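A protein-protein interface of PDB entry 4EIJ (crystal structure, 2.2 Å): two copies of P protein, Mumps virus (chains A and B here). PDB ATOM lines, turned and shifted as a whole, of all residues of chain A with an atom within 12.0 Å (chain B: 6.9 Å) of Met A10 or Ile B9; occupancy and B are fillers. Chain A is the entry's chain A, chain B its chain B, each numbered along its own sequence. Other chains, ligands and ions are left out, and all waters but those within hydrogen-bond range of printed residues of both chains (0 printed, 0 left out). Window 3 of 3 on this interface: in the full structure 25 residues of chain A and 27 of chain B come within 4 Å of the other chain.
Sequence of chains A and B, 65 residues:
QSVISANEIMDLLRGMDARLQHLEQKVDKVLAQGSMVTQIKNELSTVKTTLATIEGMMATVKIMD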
ATOM      1  N   VAL A   3     -30.055 -25.610 -19.853  1.00  0.00           N
ATOM      2  CA  VAL A   3     -28.947 -25.437 -20.791  1.00  0.00           C
ATOM      3  C   VAL A   3     -28.061 -24.245 -20.428  1.00  0.00           C
ATOM      4  O   VAL A   3     -28.519 -23.265 -19.837  1.00  0.00           O
ATOM      5  CB  VAL A   3     -29.443 -25.288 -22.249  1.00  0.00           C
ATOM      6  CG1 VAL A   3     -30.503 -24.198 -22.349  1.00  0.00           C
ATOM      7  CG2 VAL A   3     -28.278 -24.991 -23.183  1.00  0.00           C
ATOM      8  N   ILE A   4     -26.786 -24.343 -20.790  1.00  0.00           N
ATOM      9  CA  ILE A   4     -25.807 -23.301 -20.514  1.00  0.00           C
ATOM     10  C   ILE A   4     -25.887 -22.181 -21.562  1.00  0.00           C
ATOM     11  O   ILE A   4     -26.236 -22.421 -22.719  1.00  0.00           O
ATOM     12  CB  ILE A   4     -24.380 -23.902 -20.462  1.00  0.00           C
ATOM     13  CG1 ILE A   4     -23.438 -23.017 -19.645  1.00  0.00           C
ATOM     14  CG2 ILE A   4     -23.856 -24.165 -21.868  1.00  0.00           C
ATOM     15  CD1 ILE A   4     -22.053 -23.609 -19.456  1.00  0.00           C
ATOM     16  N   SER A   5     -25.586 -20.954 -21.157  1.00  0.00           N
ATOM     17  CA  SER A   5     -25.625 -19.847 -22.105  1.00  0.00           C
ATOM     18  C   SER A   5     -24.218 -19.506 -22.592  1.00  0.00           C
ATOM     19  O   SER A   5     -23.236 -19.771 -21.909  1.00  0.00           O
ATOM     20  CB  SER A   5     -26.302 -18.612 -21.500  1.00  0.00           C
ATOM     21  OG  SER A   5     -25.455 -17.965 -20.567  1.00  0.00           O
ATOM     22  N   ALA A   6     -24.140 -18.941 -23.791  1.00  0.00           N
ATOM     23  CA  ALA A   6     -22.891 -18.449 -24.352  1.00  0.00           C
ATOM     24  C   ALA A   6     -22.202 -17.491 -23.387  1.00  0.00           C
ATOM     25  O   ALA A   6     -20.989 -17.539 -23.213  1.00  0.00           O
ATOM     26  CB  ALA A   6     -23.171 -17.742 -25.669  1.00  0.00           C
ATOM     27  N   ASN A   7     -22.976 -16.603 -22.772  1.00  0.00           N
ATOM     28  CA  ASN A   7     -22.392 -15.645 -21.849  1.00  0.00           C
ATOM     29  C   ASN A   7     -21.788 -16.326 -20.635  1.00  0.00           C
ATOM     30  O   ASN A   7     -20.740 -15.918 -20.146  1.00  0.00           O
ATOM     31  CB  ASN A   7     -23.410 -14.594 -21.427  1.00  0.00           C
ATOM     32  CG  ASN A   7     -23.672 -13.587 -22.516  1.00  0.00           C
ATOM     33  OD1 ASN A   7     -22.739 -13.006 -23.069  1.00  0.00           O
ATOM     34  ND2 ASN A   7     -24.947 -13.369 -22.838  1.00  0.00           N
ATOM     35  N   GLU A   8     -22.456 -17.361 -20.142  1.00  0.00           N
ATOM     36  CA  GLU A   8     -21.934 -18.084 -18.996  1.00  0.00           C
ATOM     37  C   GLU A   8     -20.636 -18.791 -19.381  1.00  0.00           C
ATOM     38  O   GLU A   8     -19.669 -18.784 -18.617  1.00  0.00           O
ATOM     39  CB  GLU A   8     -22.965 -19.063 -18.435  1.00  0.00           C
ATOM     40  CG  GLU A   8     -22.506 -19.839 -17.194  1.00  0.00           C
ATOM     41  CD  GLU A   8     -22.227 -18.953 -15.975  1.00  0.00           C
ATOM     42  OE1 GLU A   8     -21.894 -17.759 -16.148  1.00  0.00           O
ATOM     43  OE2 GLU A   8     -22.330 -19.463 -14.835  1.00  0.00           O
ATOM     44  N   ILE A   9     -20.604 -19.380 -20.573  1.00  0.00           N
ATOM     45  CA  ILE A   9     -19.377 -20.015 -21.048  1.00  0.00           C
ATOM     46  C   ILE A   9     -18.236 -18.997 -21.123  1.00  0.00           C
ATOM     47  O   ILE A   9     -17.144 -19.271 -20.664  1.00  0.00           O
ATOM     48  CB  ILE A   9     -19.562 -20.691 -22.420  1.00  0.00           C
ATOM     49  CG1 ILE A   9     -20.486 -21.902 -22.291  1.00  0.00           C
ATOM     50  CG2 ILE A   9     -18.204 -21.114 -22.994  1.00  0.00           C
ATOM     51  CD1 ILE A   9     -20.932 -22.468 -23.631  1.00  0.00           C
ATOM     52  N   MET A  10     -18.503 -17.822 -21.685  1.00  0.00           N
ATOM     53  CA  MET A  10     -17.486 -16.785 -21.791  1.00  0.00           C
ATOM     54  C   MET A  10     -16.963 -16.379 -20.420  1.00  0.00           C
ATOM     55  O   MET A  10     -15.765 -16.171 -20.251  1.00  0.00           O
ATOM     56  CB  MET A  10     -18.010 -15.550 -22.534  1.00  0.00           C
ATOM     57  CG  MET A  10     -18.347 -15.788 -24.015  1.00  0.00           C
ATOM     58  SD  MET A  10     -19.050 -14.311 -24.792  1.00  0.00           S
ATOM     59  CE  MET A  10     -20.033 -15.042 -26.102  1.00  0.00           C
ATOM     60  N   ASP A  11     -17.859 -16.254 -19.445  1.00  0.00           N
ATOM     61  CA  ASP A  11     -17.435 -15.895 -18.097  1.00  0.00           C
ATOM     62  C   ASP A  11     -16.515 -16.949 -17.479  1.00  0.00           C
ATOM     63  O   ASP A  11     -15.511 -16.613 -16.849  1.00  0.00           O
ATOM     64  CB  ASP A  11     -18.631 -15.669 -17.173  1.00  0.00           C
ATOM     65  CG  ASP A  11     -19.433 -14.426 -17.539  1.00  0.00           C
ATOM     66  OD1 ASP A  11     -18.946 -13.604 -18.342  1.00  0.00           O
ATOM     67  OD2 ASP A  11     -20.560 -14.275 -17.008  1.00  0.00           O
ATOM     68  N   LEU A  12     -16.867 -18.221 -17.633  1.00  0.00           N
ATOM     69  CA  LEU A  12     -16.065 -19.284 -17.033  1.00  0.00           C
ATOM     70  C   LEU A  12     -14.699 -19.356 -17.709  1.00  0.00           C
ATOM     71  O   LEU A  12     -13.673 -19.475 -17.045  1.00  0.00           O
ATOM     72  CB  LEU A  12     -16.793 -20.631 -17.109  1.00  0.00           C
ATOM     73  CG  LEU A  12     -18.102 -20.737 -16.312  1.00  0.00           C
ATOM     74  CD1 LEU A  12     -18.929 -21.932 -16.763  1.00  0.00           C
ATOM     75  CD2 LEU A  12     -17.845 -20.790 -14.805  1.00  0.00           C
ATOM     76  N   LEU A  13     -14.682 -19.250 -19.035  1.00  0.00           N
ATOM     77  CA  LEU A  13     -13.411 -19.257 -19.744  1.00  0.00           C
ATOM     78  C   LEU A  13     -12.557 -18.061 -19.349  1.00  0.00           C
ATOM     79  O   LEU A  13     -11.344 -18.192 -19.199  1.00  0.00           O
ATOM     80  CB  LEU A  13     -13.618 -19.304 -21.254  1.00  0.00           C
ATOM     81  CG  LEU A  13     -14.312 -20.576 -21.752  1.00  0.00           C
ATOM     82  CD1 LEU A  13     -14.655 -20.414 -23.220  1.00  0.00           C
ATOM     83  CD2 LEU A  13     -13.431 -21.817 -21.521  1.00  0.00           C
ATOM     84  N   ARG A  14     -13.180 -16.898 -19.173  1.00  0.00           N
ATOM     85  CA  ARG A  14     -12.420 -15.717 -18.781  1.00  0.00           C
ATOM     86  C   ARG A  14     -11.793 -15.923 -17.388  1.00  0.00           C
ATOM     87  O   ARG A  14     -10.663 -15.516 -17.145  1.00  0.00           O
ATOM     88  CB  ARG A  14     -13.275 -14.445 -18.830  1.00  0.00           C
ATOM     89  CG  ARG A  14     -12.455 -13.175 -18.595  1.00  0.00           C
ATOM     90  CD  ARG A  14     -13.302 -11.905 -18.642  1.00  0.00           C
ATOM     91  NE  ARG A  14     -13.787 -11.653 -19.991  1.00  0.00           N
ATOM     92  CZ  ARG A  14     -15.023 -11.909 -20.408  1.00  0.00           C
ATOM     93  NH1 ARG A  14     -15.935 -12.416 -19.575  1.00  0.00           N
ATOM     94  NH2 ARG A  14     -15.344 -11.649 -21.666  1.00  0.00           N
ATOM     95  N   GLY A  15     -12.536 -16.570 -16.493  1.00  0.00           N
ATOM     96  CA  GLY A  15     -12.019 -16.965 -15.196  1.00  0.00           C
ATOM     97  C   GLY A  15     -10.827 -17.906 -15.290  1.00  0.00           C
ATOM     98  O   GLY A  15      -9.818 -17.695 -14.622  1.00  0.00           O
ATOM     99  N   MET A  16     -10.950 -18.946 -16.116  1.00  0.00           N
ATOM    100  CA  MET A  16      -9.865 -19.897 -16.344  1.00  0.00           C
ATOM    101  C   MET A  16      -8.636 -19.187 -16.890  1.00  0.00           C
ATOM    102  O   MET A  16      -7.513 -19.459 -16.475  1.00  0.00           O
ATOM    103  CB  MET A  16     -10.290 -20.983 -17.335  1.00  0.00           C
ATOM    104  CG  MET A  16     -11.403 -21.902 -16.850  1.00  0.00           C
ATOM    105  SD  MET A  16     -10.970 -22.869 -15.393  1.00  0.00           S
ATOM    106  CE  MET A  16     -11.491 -21.795 -14.054  1.00  0.00           C
ATOM    107  N   ASP A  17      -8.858 -18.275 -17.828  1.00  0.00           N
ATOM    108  CA  ASP A  17      -7.756 -17.550 -18.450  1.00  0.00           C
ATOM    109  C   ASP A  17      -6.993 -16.716 -17.413  1.00  0.00           C
ATOM    110  O   ASP A  17      -5.758 -16.630 -17.452  1.00  0.00           O
ATOM    111  CB  ASP A  17      -8.282 -16.682 -19.596  1.00  0.00           C
ATOM    112  CG  ASP A  17      -7.183 -15.973 -20.342  1.00  0.00           C
ATOM    113  OD1 ASP A  17      -6.404 -16.654 -21.043  1.00  0.00           O
ATOM    114  OD2 ASP A  17      -7.100 -14.731 -20.227  1.00  0.00           O
ATOM    115  N   ALA A  18      -7.722 -16.121 -16.474  1.00  0.00           N
ATOM    116  CA  ALA A  18      -7.100 -15.378 -15.383  1.00  0.00           C
ATOM    117  C   ALA A  18      -6.274 -16.285 -14.470  1.00  0.00           C
ATOM    118  O   ALA A  18      -5.215 -15.885 -13.984  1.00  0.00           O
ATOM    119  CB  ALA A  18      -8.149 -14.635 -14.569  1.00  0.00           C
ATOM    120  N   ARG A  19      -6.769 -17.494 -14.222  1.00  0.00           N
ATOM    121  CA  ARG A  19      -6.073 -18.425 -13.341  1.00  0.00           C
ATOM    122  C   ARG A  19      -4.793 -18.930 -13.990  1.00  0.00           C
ATOM    123  O   ARG A  19      -3.785 -19.092 -13.320  1.00  0.00           O
ATOM    124  CB  ARG A  19      -6.972 -19.601 -12.948  1.00  0.00           C
ATOM    125  CG  ARG A  19      -8.160 -19.199 -12.108  1.00  0.00           C
ATOM    126  CD  ARG A  19      -9.137 -20.355 -11.950  1.00  0.00           C
ATOM    127  NE  ARG A  19      -9.135 -20.870 -10.589  1.00  0.00           N
ATOM    128  CZ  ARG A  19      -9.963 -20.454  -9.642  1.00  0.00           C
ATOM    129  NH1 ARG A  19     -10.864 -19.519  -9.918  1.00  0.00           N
ATOM    130  NH2 ARG A  19      -9.893 -20.972  -8.425  1.00  0.00           N
ATOM    131  N   LEU A  20      -4.845 -19.173 -15.297  1.00  0.00           N
ATOM    132  CA  LEU A  20      -3.667 -19.591 -16.048  1.00  0.00           C
ATOM    133  C   LEU A  20      -2.592 -18.518 -15.984  1.00  0.00           C
ATOM    134  O   LEU A  20      -1.419 -18.815 -15.771  1.00  0.00           O
ATOM    135  CB  LEU A  20      -4.025 -19.873 -17.504  1.00  0.00           C
ATOM    136  CG  LEU A  20      -4.766 -21.190 -17.765  1.00  0.00           C
ATOM    137  CD1 LEU A  20      -5.228 -21.276 -19.211  1.00  0.00           C
ATOM    138  CD2 LEU A  20      -3.880 -22.382 -17.407  1.00  0.00           C
ATOM    139  N   GLN B   1     -26.274 -12.002 -33.803  1.00  0.00           N
ATOM    140  CA  GLN B   1     -25.757 -12.895 -32.778  1.00  0.00           C
ATOM    141  C   GLN B   1     -25.522 -14.294 -33.333  1.00  0.00           C
ATOM    142  O   GLN B   1     -25.476 -14.485 -34.549  1.00  0.00           O
ATOM    143  CB  GLN B   1     -26.714 -12.950 -31.582  1.00  0.00           C
ATOM    144  CG  GLN B   1     -26.250 -12.130 -30.388  1.00  0.00           C
ATOM    145  CD  GLN B   1     -24.911 -12.605 -29.850  1.00  0.00           C
ATOM    146  OE1 GLN B   1     -24.656 -13.807 -29.771  1.00  0.00           O
ATOM    147  NE2 GLN B   1     -24.049 -11.662 -29.476  1.00  0.00           N
ATOM    148  N   ILE B   4     -21.671 -14.624 -33.816  1.00  0.00           N
ATOM    149  CA  ILE B   4     -20.861 -13.671 -33.062  1.00  0.00           C
ATOM    150  C   ILE B   4     -20.426 -14.286 -31.736  1.00  0.00           C
ATOM    151  O   ILE B   4     -19.245 -14.284 -31.399  1.00  0.00           O
ATOM    152  CB  ILE B   4     -21.605 -12.350 -32.785  1.00  0.00           C
ATOM    153  CG1 ILE B   4     -21.865 -11.608 -34.097  1.00  0.00           C
ATOM    154  CG2 ILE B   4     -20.802 -11.484 -31.803  1.00  0.00           C
ATOM    155  CD1 ILE B   4     -22.613 -10.300 -33.931  1.00  0.00           C
ATOM    156  N   SER B   5     -21.387 -14.831 -31.000  1.00  0.00           N
ATOM    157  CA  SER B   5     -21.088 -15.489 -29.734  1.00  0.00           C
ATOM    158  C   SER B   5     -20.062 -16.603 -29.867  1.00  0.00           C
ATOM    159  O   SER B   5     -19.165 -16.729 -29.033  1.00  0.00           O
ATOM    160  CB  SER B   5     -22.366 -16.020 -29.077  1.00  0.00           C
ATOM    161  OG  SER B   5     -23.019 -14.974 -28.383  1.00  0.00           O
ATOM    162  N   ALA B   6     -20.195 -17.417 -30.907  1.00  0.00           N
ATOM    163  CA  ALA B   6     -19.280 -18.538 -31.081  1.00  0.00           C
ATOM    164  C   ALA B   6     -17.871 -18.042 -31.429  1.00  0.00           C
ATOM    165  O   ALA B   6     -16.875 -18.603 -30.977  1.00  0.00           O
ATOM    166  CB  ALA B   6     -19.802 -19.519 -32.130  1.00  0.00           C
ATOM    167  N   ASN B   7     -17.796 -16.989 -32.233  1.00  0.00           N
ATOM    168  CA  ASN B   7     -16.522 -16.364 -32.543  1.00  0.00           C
ATOM    169  C   ASN B   7     -15.836 -15.802 -31.296  1.00  0.00           C
ATOM    170  O   ASN B   7     -14.625 -15.924 -31.147  1.00  0.00           O
ATOM    171  CB  ASN B   7     -16.693 -15.259 -33.587  1.00  0.00           C
ATOM    172  CG  ASN B   7     -16.661 -15.794 -35.005  1.00  0.00           C
ATOM    173  OD1 ASN B   7     -17.038 -16.934 -35.259  1.00  0.00           O
ATOM    174  ND2 ASN B   7     -16.203 -14.970 -35.937  1.00  0.00           N
ATOM    175  N   GLU B   8     -16.611 -15.176 -30.414  1.00  0.00           N
ATOM    176  CA  GLU B   8     -16.059 -14.579 -29.203  1.00  0.00           C
ATOM    177  C   GLU B   8     -15.577 -15.652 -28.234  1.00  0.00           C
ATOM    178  O   GLU B   8     -14.543 -15.502 -27.596  1.00  0.00           O
ATOM    179  CB  GLU B   8     -17.071 -13.639 -28.549  1.00  0.00           C
ATOM    180  CG  GLU B   8     -17.308 -12.368 -29.374  1.00  0.00           C
ATOM    181  CD  GLU B   8     -18.413 -11.493 -28.814  1.00  0.00           C
ATOM    182  OE1 GLU B   8     -19.220 -11.997 -28.003  1.00  0.00           O
ATOM    183  OE2 GLU B   8     -18.469 -10.299 -29.187  1.00  0.00           O
ATOM    184  N   ILE B   9     -16.310 -16.752 -28.152  1.00  0.00           N
ATOM    185  CA  ILE B   9     -15.878 -17.874 -27.336  1.00  0.00           C
ATOM    186  C   ILE B   9     -14.603 -18.485 -27.924  1.00  0.00           C
ATOM    187  O   ILE B   9     -13.641 -18.724 -27.214  1.00  0.00           O
ATOM    188  CB  ILE B   9     -16.979 -18.923 -27.193  1.00  0.00           C
ATOM    189  CG1 ILE B   9     -18.097 -18.372 -26.303  1.00  0.00           C
ATOM    190  CG2 ILE B   9     -16.413 -20.211 -26.598  1.00  0.00           C
ATOM    191  CD1 ILE B   9     -19.379 -19.171 -26.341  1.00  0.00           C
ATOM    192  N   MET B  10     -14.586 -18.679 -29.232  1.00  0.00           N
ATOM    193  CA  MET B  10     -13.407 -19.182 -29.911  1.00  0.00           C
ATOM    194  C   MET B  10     -12.160 -18.307 -29.660  1.00  0.00           C
ATOM    195  O   MET B  10     -11.056 -18.835 -29.515  1.00  0.00           O
ATOM    196  CB  MET B  10     -13.672 -19.310 -31.413  1.00  0.00           C
ATOM    197  CG  MET B  10     -12.818 -20.355 -32.106  1.00  0.00           C
ATOM    198  SD  MET B  10     -13.076 -22.035 -31.473  1.00  0.00           S
ATOM    199  CE  MET B  10     -12.139 -22.979 -32.670  1.00  0.00           C
ATOM    200  N   ASP B  11     -12.331 -16.983 -29.621  1.00  0.00           N
ATOM    201  CA  ASP B  11     -11.215 -16.081 -29.310  1.00  0.00           C
ATOM    202  C   ASP B  11     -10.641 -16.311 -27.906  1.00  0.00           C
ATOM    203  O   ASP B  11      -9.433 -16.236 -27.715  1.00  0.00           O
ATOM    204  CB  ASP B  11     -11.611 -14.605 -29.459  1.00  0.00           C
ATOM    205  CG  ASP B  11     -11.711 -14.170 -30.904  1.00  0.00           C
ATOM    206  OD1 ASP B  11     -11.457 -15.003 -31.800  1.00  0.00           O
ATOM    207  OD2 ASP B  11     -12.047 -12.989 -31.144  1.00  0.00           O
ATOM    208  N   LEU B  12     -11.510 -16.575 -26.932  1.00  0.00           N
ATOM    209  CA  LEU B  12     -11.071 -16.900 -25.582  1.00  0.00           C
ATOM    210  C   LEU B  12     -10.294 -18.200 -25.598  1.00  0.00           C
ATOM    211  O   LEU B  12      -9.217 -18.292 -25.007  1.00  0.00           O
ATOM    212  CB  LEU B  12     -12.257 -17.010 -24.616  1.00  0.00           C
ATOM    213  CG  LEU B  12     -12.858 -15.638 -24.304  1.00  0.00           C
ATOM    214  CD1 LEU B  12     -14.202 -15.742 -23.613  1.00  0.00           C
ATOM    215  CD2 LEU B  12     -11.881 -14.833 -23.469  1.00  0.00           C
ATOM    216  N   LEU B  13     -10.840 -19.197 -26.289  1.00  0.00           N
ATOM    217  CA  LEU B  13     -10.192 -20.504 -26.361  1.00  0.00           C
ATOM    218  C   LEU B  13      -8.785 -20.404 -26.959  1.00  0.00           C
ATOM    219  O   LEU B  13      -7.839 -20.965 -26.414  1.00  0.00           O
ATOM    220  CB  LEU B  13     -11.061 -21.503 -27.126  1.00  0.00           C
ATOM    221  CG  LEU B  13     -12.374 -21.859 -26.407  1.00  0.00           C
ATOM    222  CD1 LEU B  13     -13.396 -22.574 -27.334  1.00  0.00           C
ATOM    223  CD2 LEU B  13     -12.082 -22.688 -25.159  1.00  0.00           C
ATOM    224  N   ARG B  14      -8.642 -19.669 -28.059  1.00  0.00           N
ATOM    225  CA  ARG B  14      -7.338 -19.537 -28.703  1.00  0.00           C
ATOM    226  C   ARG B  14      -6.343 -18.784 -27.821  1.00  0.00           C
ATOM    227  O   ARG B  14      -5.147 -19.079 -27.844  1.00  0.00           O
ATOM    228  CB  ARG B  14      -7.452 -18.857 -30.071  1.00  0.00           C
ATOM    229  CG  ARG B  14      -8.286 -19.620 -31.085  1.00  0.00           C
ATOM    230  CD  ARG B  14      -8.018 -19.098 -32.482  1.00  0.00           C
ATOM    231  NE  ARG B  14      -9.062 -19.464 -33.434  1.00  0.00           N
ATOM    232  CZ  ARG B  14     -10.109 -18.698 -33.721  1.00  0.00           C
ATOM    233  NH1 ARG B  14     -10.261 -17.523 -33.122  1.00  0.00           N
ATOM    234  NH2 ARG B  14     -11.007 -19.108 -34.604  1.00  0.00           N
ATOM    235  N   GLY B  15      -6.830 -17.805 -27.060  1.00  0.00           N
ATOM    236  CA  GLY B  15      -5.964 -17.075 -26.146  1.00  0.00           C
ATOM    237  C   GLY B  15      -5.472 -18.021 -25.062  1.00  0.00           C
ATOM    238  O   GLY B  15      -4.321 -17.962 -24.632  1.00  0.00           O
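OE1 of Gln B1 lies within hydrogen-bond range of OG of Ser B5, at 2.4 Å.
Among the printed residues, pairs that only touch across the chains: Met A10 with Ile B9, Met A10 with Ser B5, Met A10 with Glu B8, Met A10 with Leu B12, Leu A13 with Ile B9, Ala A6 with Ile B9, Ala A6 with Ser B5 and Leu A13 with Leu B13.
Printed residues of chain B within 4 Å of Ala A6: Ser B5 and Ile B9. Met A10 touches four residues of chain B. Asp A11 touches none of the printed residues of chain B. Of the printed residues of chain B, Leu A13 touches Ile B9 and Leu B13. Arg A19 touches none of the printed residues of chain B. No residue of chain A comes within 4 Å of Ala B6. Printed residues of chain A within 4 Å of Ile B9: Ala A6 (3.9 Å), Met A10 (3.5 Å) and Leu A13 (3.8 Å). Met B10 touches none of the printed residues of chain A. No residue of chain A comes within 4 Å of Asp B11. Leu B12 touches just one residue of chain A: Met A10 (3.7 Å). Leu B13 touches just one residue of chain A: Leu A13.
Of the 13 printed residues of chain B, 5 touch a printed residue of chain A. Printed residues of chain A that touch a printed residue of chain B: Ala A6, Met A10 and Leu A13.
Ala A6 touches Ile B9, but with the chains exchanged Ile A9 does not touch Ala B6 (8.5 Å). Met A10 touches Ser B5, but with the chains exchanged Ser A5 does not touch Met B10 (11.4 Å). Leu A13 touches Ile B9, but with the chains exchanged Ile A9 does not touch Leu B13 (6.6 Å). Leu B13 touches its own counterpart, Leu A13. 12 positions are printed for both chains.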
